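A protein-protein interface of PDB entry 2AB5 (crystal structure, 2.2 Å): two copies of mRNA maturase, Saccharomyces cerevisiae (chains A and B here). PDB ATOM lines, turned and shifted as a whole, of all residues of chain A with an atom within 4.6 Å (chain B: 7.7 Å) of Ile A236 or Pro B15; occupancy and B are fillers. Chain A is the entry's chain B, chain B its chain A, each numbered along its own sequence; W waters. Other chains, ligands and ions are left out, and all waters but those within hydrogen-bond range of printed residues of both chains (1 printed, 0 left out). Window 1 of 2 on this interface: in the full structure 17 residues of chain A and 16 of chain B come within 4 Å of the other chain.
The side-chain amino group (NZ) of Lys A237 is in hydrogen-bond range of the side-chain amide oxygen (OD1) of Asn B151 (2.6 Å).
N of Ile B16 sits close to ND2 of Asn B14. N of Ile A236 sits at hydrogen-bond distance from OD1 of Asn A234 (2.8 Å).
Among the printed residues, pairs that only touch across the chains: Pro A15 with Pro B235 (2.9 Å), Ile A16 with Asn B14 (3.6 Å), Ser A155 with Pro B235 (3.8 Å), Pro A235 with Pro B15 (3.6 Å), Pro A235 with Ser B155 (3.6 Å), Pro A235 with Pro B235 (3.5 Å) and Ile A236 with Pro B15 (3.9 Å).
Of chain B, only Pro B15 comes within 4 Å of Ile A236. Of chain A, only Pro A235 and Ile A236 come within 4 Å of Pro B15. Printed residues of chain B within 4 Å of Lys A237: Asn B151 (2.6 Å). Of the printed residues of chain B, Ile A16 touches Asn B14 (3.6 Å). Of the printed residues of chain B, Ser A155 touches Pro B235. Of the printed residues of chain B, Pro A15 touches Pro B235. Printed residues of chain A within 4 Å of Pro B235: Pro A15 (2.9 Å), Ser A155 (3.8 Å) and Pro A235 (3.5 Å). Ile A158 touches none of the printed residues of chain B. Tyr B152 touches none of the printed residues of chain A.
Of the 10 printed residues of chain A, 6 touch a printed residue of chain B. Printed residues of chain A that touch a printed residue of chain B: Pro A15, Ile A16, Ser A155, Pro A235, Ile A236 and Lys A237. Hydrophobic or aromatic side chains of chain A within 4 Å of the printed part of chain B: Pro A15, Ile A16, Pro A235 and Ile A236. Among the printed residues, 8 pairs touch across the chains. Among the printed residues, no Asp or Glu carboxylate lies within 4 Å of a Lys or Arg side-chain nitrogen of the other chain.
Pro A15 touches Pro B235, and with the chains exchanged Pro A235 touches Pro B15. Ser A155 touches Pro B235, and with the chains exchanged Pro A235 touches Ser B155. Pro B235 touches its own counterpart, Pro A235. Ile A236 touches Pro B15, but with the chains exchanged Pro A15 does not touch Ile B236 (4.2 Å). Positions printed for both chains: 15, 16, 19, 155, 234, 235 and 236.
Water W1 lies within hydrogen-bond range of N of Lys A237 (3.1 Å) and O of Asp B13 (3.2 Å).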
ATOM      1  N   PRO A  15     -19.924 -22.147  16.740  1.00  0.00           N
ATOM      2  CA  PRO A  15     -18.732 -21.936  15.909  1.00  0.00           C
ATOM      3  C   PRO A  15     -17.609 -22.957  16.080  1.00  0.00           C
ATOM      4  O   PRO A  15     -16.847 -23.189  15.157  1.00  0.00           O
ATOM      5  CB  PRO A  15     -18.259 -20.530  16.314  1.00  0.00           C
ATOM      6  CG  PRO A  15     -19.457 -19.875  16.800  1.00  0.00           C
ATOM      7  CD  PRO A  15     -20.175 -20.963  17.575  1.00  0.00           C
ATOM      8  N   ILE A  16     -17.486 -23.570  17.255  1.00  0.00           N
ATOM      9  CA  ILE A  16     -16.402 -24.524  17.424  1.00  0.00           C
ATOM     10  C   ILE A  16     -16.556 -25.723  16.491  1.00  0.00           C
ATOM     11  O   ILE A  16     -15.592 -26.442  16.227  1.00  0.00           O
ATOM     12  CB  ILE A  16     -16.279 -25.000  18.886  1.00  0.00           C
ATOM     13  CG1 ILE A  16     -14.872 -25.569  19.101  1.00  0.00           C
ATOM     14  CG2 ILE A  16     -17.331 -26.071  19.194  1.00  0.00           C
ATOM     15  CD1 ILE A  16     -14.373 -25.396  20.479  1.00  0.00           C
ATOM     16  N   TYR A  19     -14.659 -24.933  13.598  1.00  0.00           N
ATOM     17  CA  TYR A  19     -13.256 -25.154  13.917  1.00  0.00           C
ATOM     18  C   TYR A  19     -12.965 -26.639  13.705  1.00  0.00           C
ATOM     19  O   TYR A  19     -11.914 -27.015  13.174  1.00  0.00           O
ATOM     20  CB  TYR A  19     -12.979 -24.756  15.377  1.00  0.00           C
ATOM     21  CG  TYR A  19     -11.799 -25.469  15.999  1.00  0.00           C
ATOM     22  CD1 TYR A  19     -10.503 -24.946  15.906  1.00  0.00           C
ATOM     23  CD2 TYR A  19     -11.973 -26.688  16.669  1.00  0.00           C
ATOM     24  CE1 TYR A  19      -9.399 -25.626  16.478  1.00  0.00           C
ATOM     25  CE2 TYR A  19     -10.898 -27.372  17.226  1.00  0.00           C
ATOM     26  CZ  TYR A  19      -9.614 -26.839  17.134  1.00  0.00           C
ATOM     27  OH  TYR A  19      -8.554 -27.502  17.705  1.00  0.00           O
ATOM     28  N   SER A 155     -13.587 -18.992  11.909  1.00  0.00           N
ATOM     29  CA  SER A 155     -13.622 -20.119  12.852  1.00  0.00           C
ATOM     30  C   SER A 155     -13.025 -21.351  12.204  1.00  0.00           C
ATOM     31  O   SER A 155     -12.294 -22.106  12.841  1.00  0.00           O
ATOM     32  CB  SER A 155     -15.057 -20.437  13.300  1.00  0.00           C
ATOM     33  OG  SER A 155     -15.587 -19.411  14.124  1.00  0.00           O
ATOM     34  N   ILE A 158      -9.146 -21.257  12.289  1.00  0.00           N
ATOM     35  CA  ILE A 158      -8.368 -21.620  13.470  1.00  0.00           C
ATOM     36  C   ILE A 158      -8.175 -23.132  13.492  1.00  0.00           C
ATOM     37  O   ILE A 158      -7.140 -23.639  13.931  1.00  0.00           O
ATOM     38  CB  ILE A 158      -9.065 -21.154  14.769  1.00  0.00           C
ATOM     39  CG1 ILE A 158      -9.111 -19.627  14.801  1.00  0.00           C
ATOM     40  CG2 ILE A 158      -8.316 -21.671  16.001  1.00  0.00           C
ATOM     41  CD1 ILE A 158      -7.725 -18.966  14.759  1.00  0.00           C
ATOM     42  N   ASN A 234      -9.463 -13.776  18.319  1.00  0.00           N
ATOM     43  CA  ASN A 234     -10.514 -14.713  17.936  1.00  0.00           C
ATOM     44  C   ASN A 234     -10.984 -15.497  19.153  1.00  0.00           C
ATOM     45  O   ASN A 234     -10.169 -16.034  19.893  1.00  0.00           O
ATOM     46  CB  ASN A 234      -9.999 -15.698  16.879  1.00  0.00           C
ATOM     47  CG  ASN A 234     -11.125 -16.408  16.154  1.00  0.00           C
ATOM     48  OD1 ASN A 234     -12.113 -16.784  16.766  1.00  0.00           O
ATOM     49  ND2 ASN A 234     -10.979 -16.591  14.845  1.00  0.00           N
ATOM     50  N   PRO A 235     -12.305 -15.566  19.383  1.00  0.00           N
ATOM     51  CA  PRO A 235     -12.814 -16.314  20.541  1.00  0.00           C
ATOM     52  C   PRO A 235     -12.636 -17.817  20.354  1.00  0.00           C
ATOM     53  O   PRO A 235     -12.681 -18.571  21.323  1.00  0.00           O
ATOM     54  CB  PRO A 235     -14.279 -15.887  20.609  1.00  0.00           C
ATOM     55  CG  PRO A 235     -14.612 -15.678  19.194  1.00  0.00           C
ATOM     56  CD  PRO A 235     -13.413 -14.910  18.672  1.00  0.00           C
ATOM     57  N   ILE A 236     -12.450 -18.243  19.103  1.00  0.00           N
ATOM     58  CA  ILE A 236     -12.223 -19.647  18.791  1.00  0.00           C
ATOM     59  C   ILE A 236     -10.708 -19.835  18.916  1.00  0.00           C
ATOM     60  O   ILE A 236      -9.936 -19.113  18.279  1.00  0.00           O
ATOM     61  CB  ILE A 236     -12.695 -19.993  17.369  1.00  0.00           C
ATOM     62  CG1 ILE A 236     -14.235 -19.942  17.298  1.00  0.00           C
ATOM     63  CG2 ILE A 236     -12.230 -21.388  17.004  1.00  0.00           C
ATOM     64  CD1 ILE A 236     -14.957 -20.998  18.190  1.00  0.00           C
ATOM     65  N   LYS A 237     -10.280 -20.798  19.731  1.00  0.00           N
ATOM     66  CA  LYS A 237      -8.854 -20.976  19.978  1.00  0.00           C
ATOM     67  C   LYS A 237      -8.147 -22.258  19.577  1.00  0.00           C
ATOM     68  O   LYS A 237      -8.772 -23.297  19.368  1.00  0.00           O
ATOM     69  CB  LYS A 237      -8.592 -20.738  21.470  1.00  0.00           C
ATOM     70  CG  LYS A 237      -9.018 -19.369  21.942  1.00  0.00           C
ATOM     71  CD  LYS A 237      -8.501 -19.084  23.329  1.00  0.00           C
ATOM     72  CE  LYS A 237      -8.718 -17.625  23.683  1.00  0.00           C
ATOM     73  NZ  LYS A 237      -7.858 -17.178  24.820  1.00  0.00           N
ATOM     74  N   LEU A 238      -6.820 -22.160  19.476  1.00  0.00           N
ATOM     75  CA  LEU A 238      -5.972 -23.312  19.181  1.00  0.00           C
ATOM     76  C   LEU A 238      -6.075 -24.163  20.455  1.00  0.00           C
ATOM     77  O   LEU A 238      -6.005 -23.629  21.555  1.00  0.00           O
ATOM     78  CB  LEU A 238      -4.528 -22.866  18.967  1.00  0.00           C
ATOM     79  CG  LEU A 238      -4.316 -21.940  17.774  1.00  0.00           C
ATOM     80  CD1 LEU A 238      -2.899 -21.404  17.807  1.00  0.00           C
ATOM     81  CD2 LEU A 238      -4.593 -22.701  16.468  1.00  0.00           C
ATOM     82  N   THR B  12     -14.607 -27.550  28.453  1.00  0.00           N
ATOM     83  CA  THR B  12     -15.135 -26.192  28.479  1.00  0.00           C
ATOM     84  C   THR B  12     -14.392 -25.191  27.572  1.00  0.00           C
ATOM     85  O   THR B  12     -14.350 -23.983  27.849  1.00  0.00           O
ATOM     86  CB  THR B  12     -15.140 -25.657  29.938  1.00  0.00           C
ATOM     87  OG1 THR B  12     -13.808 -25.714  30.471  1.00  0.00           O
ATOM     88  CG2 THR B  12     -16.078 -26.501  30.829  1.00  0.00           C
ATOM     89  N   ASP B  13     -13.822 -25.694  26.485  1.00  0.00           N
ATOM     90  CA  ASP B  13     -13.093 -24.853  25.537  1.00  0.00           C
ATOM     91  C   ASP B  13     -13.983 -24.038  24.608  1.00  0.00           C
ATOM     92  O   ASP B  13     -13.508 -23.126  23.945  1.00  0.00           O
ATOM     93  CB  ASP B  13     -12.184 -25.718  24.676  1.00  0.00           C
ATOM     94  CG  ASP B  13     -11.064 -26.305  25.462  1.00  0.00           C
ATOM     95  OD1 ASP B  13     -10.426 -25.509  26.175  1.00  0.00           O
ATOM     96  OD2 ASP B  13     -10.830 -27.531  25.363  1.00  0.00           O
ATOM     97  N   ASN B  14     -15.264 -24.382  24.558  1.00  0.00           N
ATOM     98  CA  ASN B  14     -16.195 -23.698  23.678  1.00  0.00           C
ATOM     99  C   ASN B  14     -16.645 -22.347  24.219  1.00  0.00           C
ATOM    100  O   ASN B  14     -17.271 -22.264  25.275  1.00  0.00           O
ATOM    101  CB  ASN B  14     -17.403 -24.604  23.417  1.00  0.00           C
ATOM    102  CG  ASN B  14     -18.304 -24.080  22.313  1.00  0.00           C
ATOM    103  OD1 ASN B  14     -19.269 -24.742  21.940  1.00  0.00           O
ATOM    104  ND2 ASN B  14     -18.002 -22.887  21.791  1.00  0.00           N
ATOM    105  N   PRO B  15     -16.326 -21.261  23.493  1.00  0.00           N
ATOM    106  CA  PRO B  15     -16.725 -19.927  23.945  1.00  0.00           C
ATOM    107  C   PRO B  15     -18.239 -19.727  23.974  1.00  0.00           C
ATOM    108  O   PRO B  15     -18.702 -18.718  24.478  1.00  0.00           O
ATOM    109  CB  PRO B  15     -16.033 -18.996  22.939  1.00  0.00           C
ATOM    110  CG  PRO B  15     -16.074 -19.788  21.694  1.00  0.00           C
ATOM    111  CD  PRO B  15     -15.645 -21.176  22.190  1.00  0.00           C
ATOM    112  N   ILE B  16     -19.020 -20.666  23.434  1.00  0.00           N
ATOM    113  CA  ILE B  16     -20.469 -20.454  23.475  1.00  0.00           C
ATOM    114  C   ILE B  16     -20.984 -20.608  24.914  1.00  0.00           C
ATOM    115  O   ILE B  16     -22.080 -20.149  25.260  1.00  0.00           O
ATOM    116  CB  ILE B  16     -21.231 -21.391  22.493  1.00  0.00           C
ATOM    117  CG1 ILE B  16     -22.647 -20.830  22.279  1.00  0.00           C
ATOM    118  CG2 ILE B  16     -21.243 -22.837  23.009  1.00  0.00           C
ATOM    119  CD1 ILE B  16     -23.312 -21.316  21.019  1.00  0.00           C
ATOM    120  N   TYR B  17     -20.164 -21.226  25.760  1.00  0.00           N
ATOM    121  CA  TYR B  17     -20.503 -21.403  27.178  1.00  0.00           C
ATOM    122  C   TYR B  17     -20.376 -20.053  27.876  1.00  0.00           C
ATOM    123  O   TYR B  17     -21.036 -19.795  28.882  1.00  0.00           O
ATOM    124  CB  TYR B  17     -19.566 -22.425  27.837  1.00  0.00           C
ATOM    125  CG  TYR B  17     -19.828 -23.875  27.462  1.00  0.00           C
ATOM    126  CD1 TYR B  17     -18.791 -24.819  27.480  1.00  0.00           C
ATOM    127  CD2 TYR B  17     -21.116 -24.323  27.138  1.00  0.00           C
ATOM    128  CE1 TYR B  17     -19.026 -26.174  27.188  1.00  0.00           C
ATOM    129  CE2 TYR B  17     -21.365 -25.682  26.844  1.00  0.00           C
ATOM    130  CZ  TYR B  17     -20.312 -26.595  26.875  1.00  0.00           C
ATOM    131  OH  TYR B  17     -20.540 -27.931  26.623  1.00  0.00           O
ATOM    132  N   ALA B  18     -19.515 -19.186  27.350  1.00  0.00           N
ATOM    133  CA  ALA B  18     -19.342 -17.841  27.931  1.00  0.00           C
ATOM    134  C   ALA B  18     -20.554 -17.017  27.525  1.00  0.00           C
ATOM    135  O   ALA B  18     -20.997 -16.128  28.252  1.00  0.00           O
ATOM    136  CB  ALA B  18     -18.069 -17.187  27.401  1.00  0.00           C
ATOM    137  N   TYR B  19     -21.071 -17.308  26.333  1.00  0.00           N
ATOM    138  CA  TYR B  19     -22.249 -16.631  25.832  1.00  0.00           C
ATOM    139  C   TYR B  19     -23.397 -17.079  26.741  1.00  0.00           C
ATOM    140  O   TYR B  19     -24.217 -16.267  27.161  1.00  0.00           O
ATOM    141  CB  TYR B  19     -22.508 -17.035  24.371  1.00  0.00           C
ATOM    142  CG  TYR B  19     -23.953 -16.929  23.972  1.00  0.00           C
ATOM    143  CD1 TYR B  19     -24.482 -15.736  23.473  1.00  0.00           C
ATOM    144  CD2 TYR B  19     -24.807 -18.018  24.117  1.00  0.00           C
ATOM    145  CE1 TYR B  19     -25.844 -15.642  23.126  1.00  0.00           C
ATOM    146  CE2 TYR B  19     -26.148 -17.937  23.781  1.00  0.00           C
ATOM    147  CZ  TYR B  19     -26.665 -16.753  23.280  1.00  0.00           C
ATOM    148  OH  TYR B  19     -27.988 -16.710  22.891  1.00  0.00           O
ATOM    149  N   ILE B  20     -23.451 -18.375  27.052  1.00  0.00           N
ATOM    150  CA  ILE B  20     -24.496 -18.886  27.940  1.00  0.00           C
ATOM    151  C   ILE B  20     -24.433 -18.168  29.293  1.00  0.00           C
ATOM    152  O   ILE B  20     -25.453 -17.710  29.802  1.00  0.00           O
ATOM    153  CB  ILE B  20     -24.358 -20.422  28.204  1.00  0.00           C
ATOM    154  CG1 ILE B  20     -24.610 -21.221  26.922  1.00  0.00           C
ATOM    155  CG2 ILE B  20     -25.361 -20.853  29.281  1.00  0.00           C
ATOM    156  CD1 ILE B  20     -25.974 -21.007  26.330  1.00  0.00           C
ATOM    157  N   VAL B  21     -23.243 -18.071  29.880  1.00  0.00           N
ATOM    158  CA  VAL B  21     -23.111 -17.389  31.166  1.00  0.00           C
ATOM    159  C   VAL B  21     -23.585 -15.948  31.032  1.00  0.00           C
ATOM    160  O   VAL B  21     -24.259 -15.409  31.916  1.00  0.00           O
ATOM    161  CB  VAL B  21     -21.627 -17.396  31.684  1.00  0.00           C
ATOM    162  CG1 VAL B  21     -21.479 -16.453  32.874  1.00  0.00           C
ATOM    163  CG2 VAL B  21     -21.220 -18.801  32.105  1.00  0.00           C
ATOM    164  N   TYR B 104     -16.000 -19.791  32.859  1.00  0.00           N
ATOM    165  CA  TYR B 104     -16.396 -18.447  32.442  1.00  0.00           C
ATOM    166  C   TYR B 104     -17.229 -17.724  33.490  1.00  0.00           C
ATOM    167  O   TYR B 104     -18.425 -17.516  33.307  1.00  0.00           O
ATOM    168  CB  TYR B 104     -17.180 -18.521  31.129  1.00  0.00           C
ATOM    169  CG  TYR B 104     -16.415 -19.196  30.010  1.00  0.00           C
ATOM    170  CD1 TYR B 104     -16.828 -20.428  29.502  1.00  0.00           C
ATOM    171  CD2 TYR B 104     -15.284 -18.595  29.445  1.00  0.00           C
ATOM    172  CE1 TYR B 104     -16.147 -21.040  28.465  1.00  0.00           C
ATOM    173  CE2 TYR B 104     -14.588 -19.210  28.396  1.00  0.00           C
ATOM    174  CZ  TYR B 104     -15.028 -20.429  27.916  1.00  0.00           C
ATOM    175  OH  TYR B 104     -14.352 -21.060  26.906  1.00  0.00           O
ATOM    176  N   ASN B 151     -10.404 -12.575  28.813  1.00  0.00           N
ATOM    177  CA  ASN B 151     -10.321 -12.915  27.408  1.00  0.00           C
ATOM    178  C   ASN B 151     -11.589 -13.546  26.826  1.00  0.00           C
ATOM    179  O   ASN B 151     -11.572 -14.025  25.699  1.00  0.00           O
ATOM    180  CB  ASN B 151      -9.145 -13.864  27.164  1.00  0.00           C
ATOM    181  CG  ASN B 151      -9.459 -15.303  27.555  1.00  0.00           C
ATOM    182  OD1 ASN B 151      -8.830 -16.243  27.058  1.00  0.00           O
ATOM    183  ND2 ASN B 151     -10.427 -15.483  28.450  1.00  0.00           N
ATOM    184  N   TYR B 152     -12.679 -13.574  27.583  1.00  0.00           N
ATOM    185  CA  TYR B 152     -13.916 -14.153  27.074  1.00  0.00           C
ATOM    186  C   TYR B 152     -15.024 -13.127  27.181  1.00  0.00           C
ATOM    187  O   TYR B 152     -16.197 -13.462  27.046  1.00  0.00           O
ATOM    188  CB  TYR B 152     -14.299 -15.404  27.870  1.00  0.00           C
ATOM    189  CG  TYR B 152     -14.595 -15.128  29.319  1.00  0.00           C
ATOM    190  CD1 TYR B 152     -15.850 -14.694  29.724  1.00  0.00           C
ATOM    191  CD2 TYR B 152     -13.605 -15.285  30.291  1.00  0.00           C
ATOM    192  CE1 TYR B 152     -16.120 -14.420  31.075  1.00  0.00           C
ATOM    193  CE2 TYR B 152     -13.861 -15.013  31.637  1.00  0.00           C
ATOM    194  CZ  TYR B 152     -15.118 -14.583  32.023  1.00  0.00           C
ATOM    195  OH  TYR B 152     -15.366 -14.326  33.353  1.00  0.00           O
ATOM    196  N   SER B 154     -15.881 -10.639  25.157  1.00  0.00           N
ATOM    197  CA  SER B 154     -16.644 -10.424  23.938  1.00  0.00           C
ATOM    198  C   SER B 154     -17.720 -11.491  23.698  1.00  0.00           C
ATOM    199  O   SER B 154     -18.742 -11.198  23.088  1.00  0.00           O
ATOM    200  CB  SER B 154     -15.694 -10.325  22.738  1.00  0.00           C
ATOM    201  OG  SER B 154     -15.106 -11.567  22.417  1.00  0.00           O
ATOM    202  N   SER B 155     -17.494 -12.714  24.181  1.00  0.00           N
ATOM    203  CA  SER B 155     -18.456 -13.814  24.016  1.00  0.00           C
ATOM    204  C   SER B 155     -19.553 -13.669  25.065  1.00  0.00           C
ATOM    205  O   SER B 155     -20.728 -13.934  24.811  1.00  0.00           O
ATOM    206  CB  SER B 155     -17.766 -15.177  24.167  1.00  0.00           C
ATOM    207  OG  SER B 155     -16.818 -15.433  23.129  1.00  0.00           O
ATOM    208  N   TRP B 156     -19.149 -13.254  26.259  1.00  0.00           N
ATOM    209  CA  TRP B 156     -20.087 -13.021  27.343  1.00  0.00           C
ATOM    210  C   TRP B 156     -21.007 -11.874  26.900  1.00  0.00           C
ATOM    211  O   TRP B 156     -22.233 -11.914  27.096  1.00  0.00           O
ATOM    212  CB  TRP B 156     -19.316 -12.605  28.607  1.00  0.00           C
ATOM    213  CG  TRP B 156     -20.178 -12.213  29.769  1.00  0.00           C
ATOM    214  CD1 TRP B 156     -20.634 -13.028  30.772  1.00  0.00           C
ATOM    215  CD2 TRP B 156     -20.708 -10.910  30.039  1.00  0.00           C
ATOM    216  NE1 TRP B 156     -21.413 -12.309  31.649  1.00  0.00           N
ATOM    217  CE2 TRP B 156     -21.475 -11.007  31.223  1.00  0.00           C
ATOM    218  CE3 TRP B 156     -20.609  -9.666  29.398  1.00  0.00           C
ATOM    219  CZ2 TRP B 156     -22.138  -9.908  31.775  1.00  0.00           C
ATOM    220  CZ3 TRP B 156     -21.270  -8.577  29.945  1.00  0.00           C
ATOM    221  CH2 TRP B 156     -22.024  -8.704  31.121  1.00  0.00           C
ATOM    222  N   ASN B 234     -18.394 -10.755  15.257  1.00  0.00           N
ATOM    223  CA  ASN B 234     -18.217 -11.750  16.303  1.00  0.00           C
ATOM    224  C   ASN B 234     -18.652 -13.132  15.817  1.00  0.00           C
ATOM    225  O   ASN B 234     -19.711 -13.271  15.226  1.00  0.00           O
ATOM    226  CB  ASN B 234     -19.043 -11.332  17.522  1.00  0.00           C
ATOM    227  CG  ASN B 234     -18.539 -11.949  18.807  1.00  0.00           C
ATOM    228  OD1 ASN B 234     -18.217 -13.131  18.852  1.00  0.00           O
ATOM    229  ND2 ASN B 234     -18.496 -11.156  19.861  1.00  0.00           N
ATOM    230  N   PRO B 235     -17.824 -14.172  16.035  1.00  0.00           N
ATOM    231  CA  PRO B 235     -18.174 -15.536  15.608  1.00  0.00           C
ATOM    232  C   PRO B 235     -19.304 -16.090  16.488  1.00  0.00           C
ATOM    233  O   PRO B 235     -19.961 -17.053  16.126  1.00  0.00           O
ATOM    234  CB  PRO B 235     -16.883 -16.323  15.828  1.00  0.00           C
ATOM    235  CG  PRO B 235     -15.813 -15.250  15.857  1.00  0.00           C
ATOM    236  CD  PRO B 235     -16.467 -14.141  16.602  1.00  0.00           C
ATOM    237  N   ILE B 236     -19.481 -15.480  17.656  1.00  0.00           N
ATOM    238  CA  ILE B 236     -20.510 -15.848  18.628  1.00  0.00           C
ATOM    239  C   ILE B 236     -21.709 -14.969  18.285  1.00  0.00           C
ATOM    240  O   ILE B 236     -21.604 -13.744  18.296  1.00  0.00           O
ATOM    241  CB  ILE B 236     -20.019 -15.551  20.067  1.00  0.00           C
ATOM    242  CG1 ILE B 236     -18.856 -16.491  20.416  1.00  0.00           C
ATOM    243  CG2 ILE B 236     -21.184 -15.682  21.062  1.00  0.00           C
ATOM    244  CD1 ILE B 236     -19.257 -17.994  20.516  1.00  0.00           C
HETATM  245  O   HOH W   1     -12.582 -22.455  20.947  1.00  0.00           O
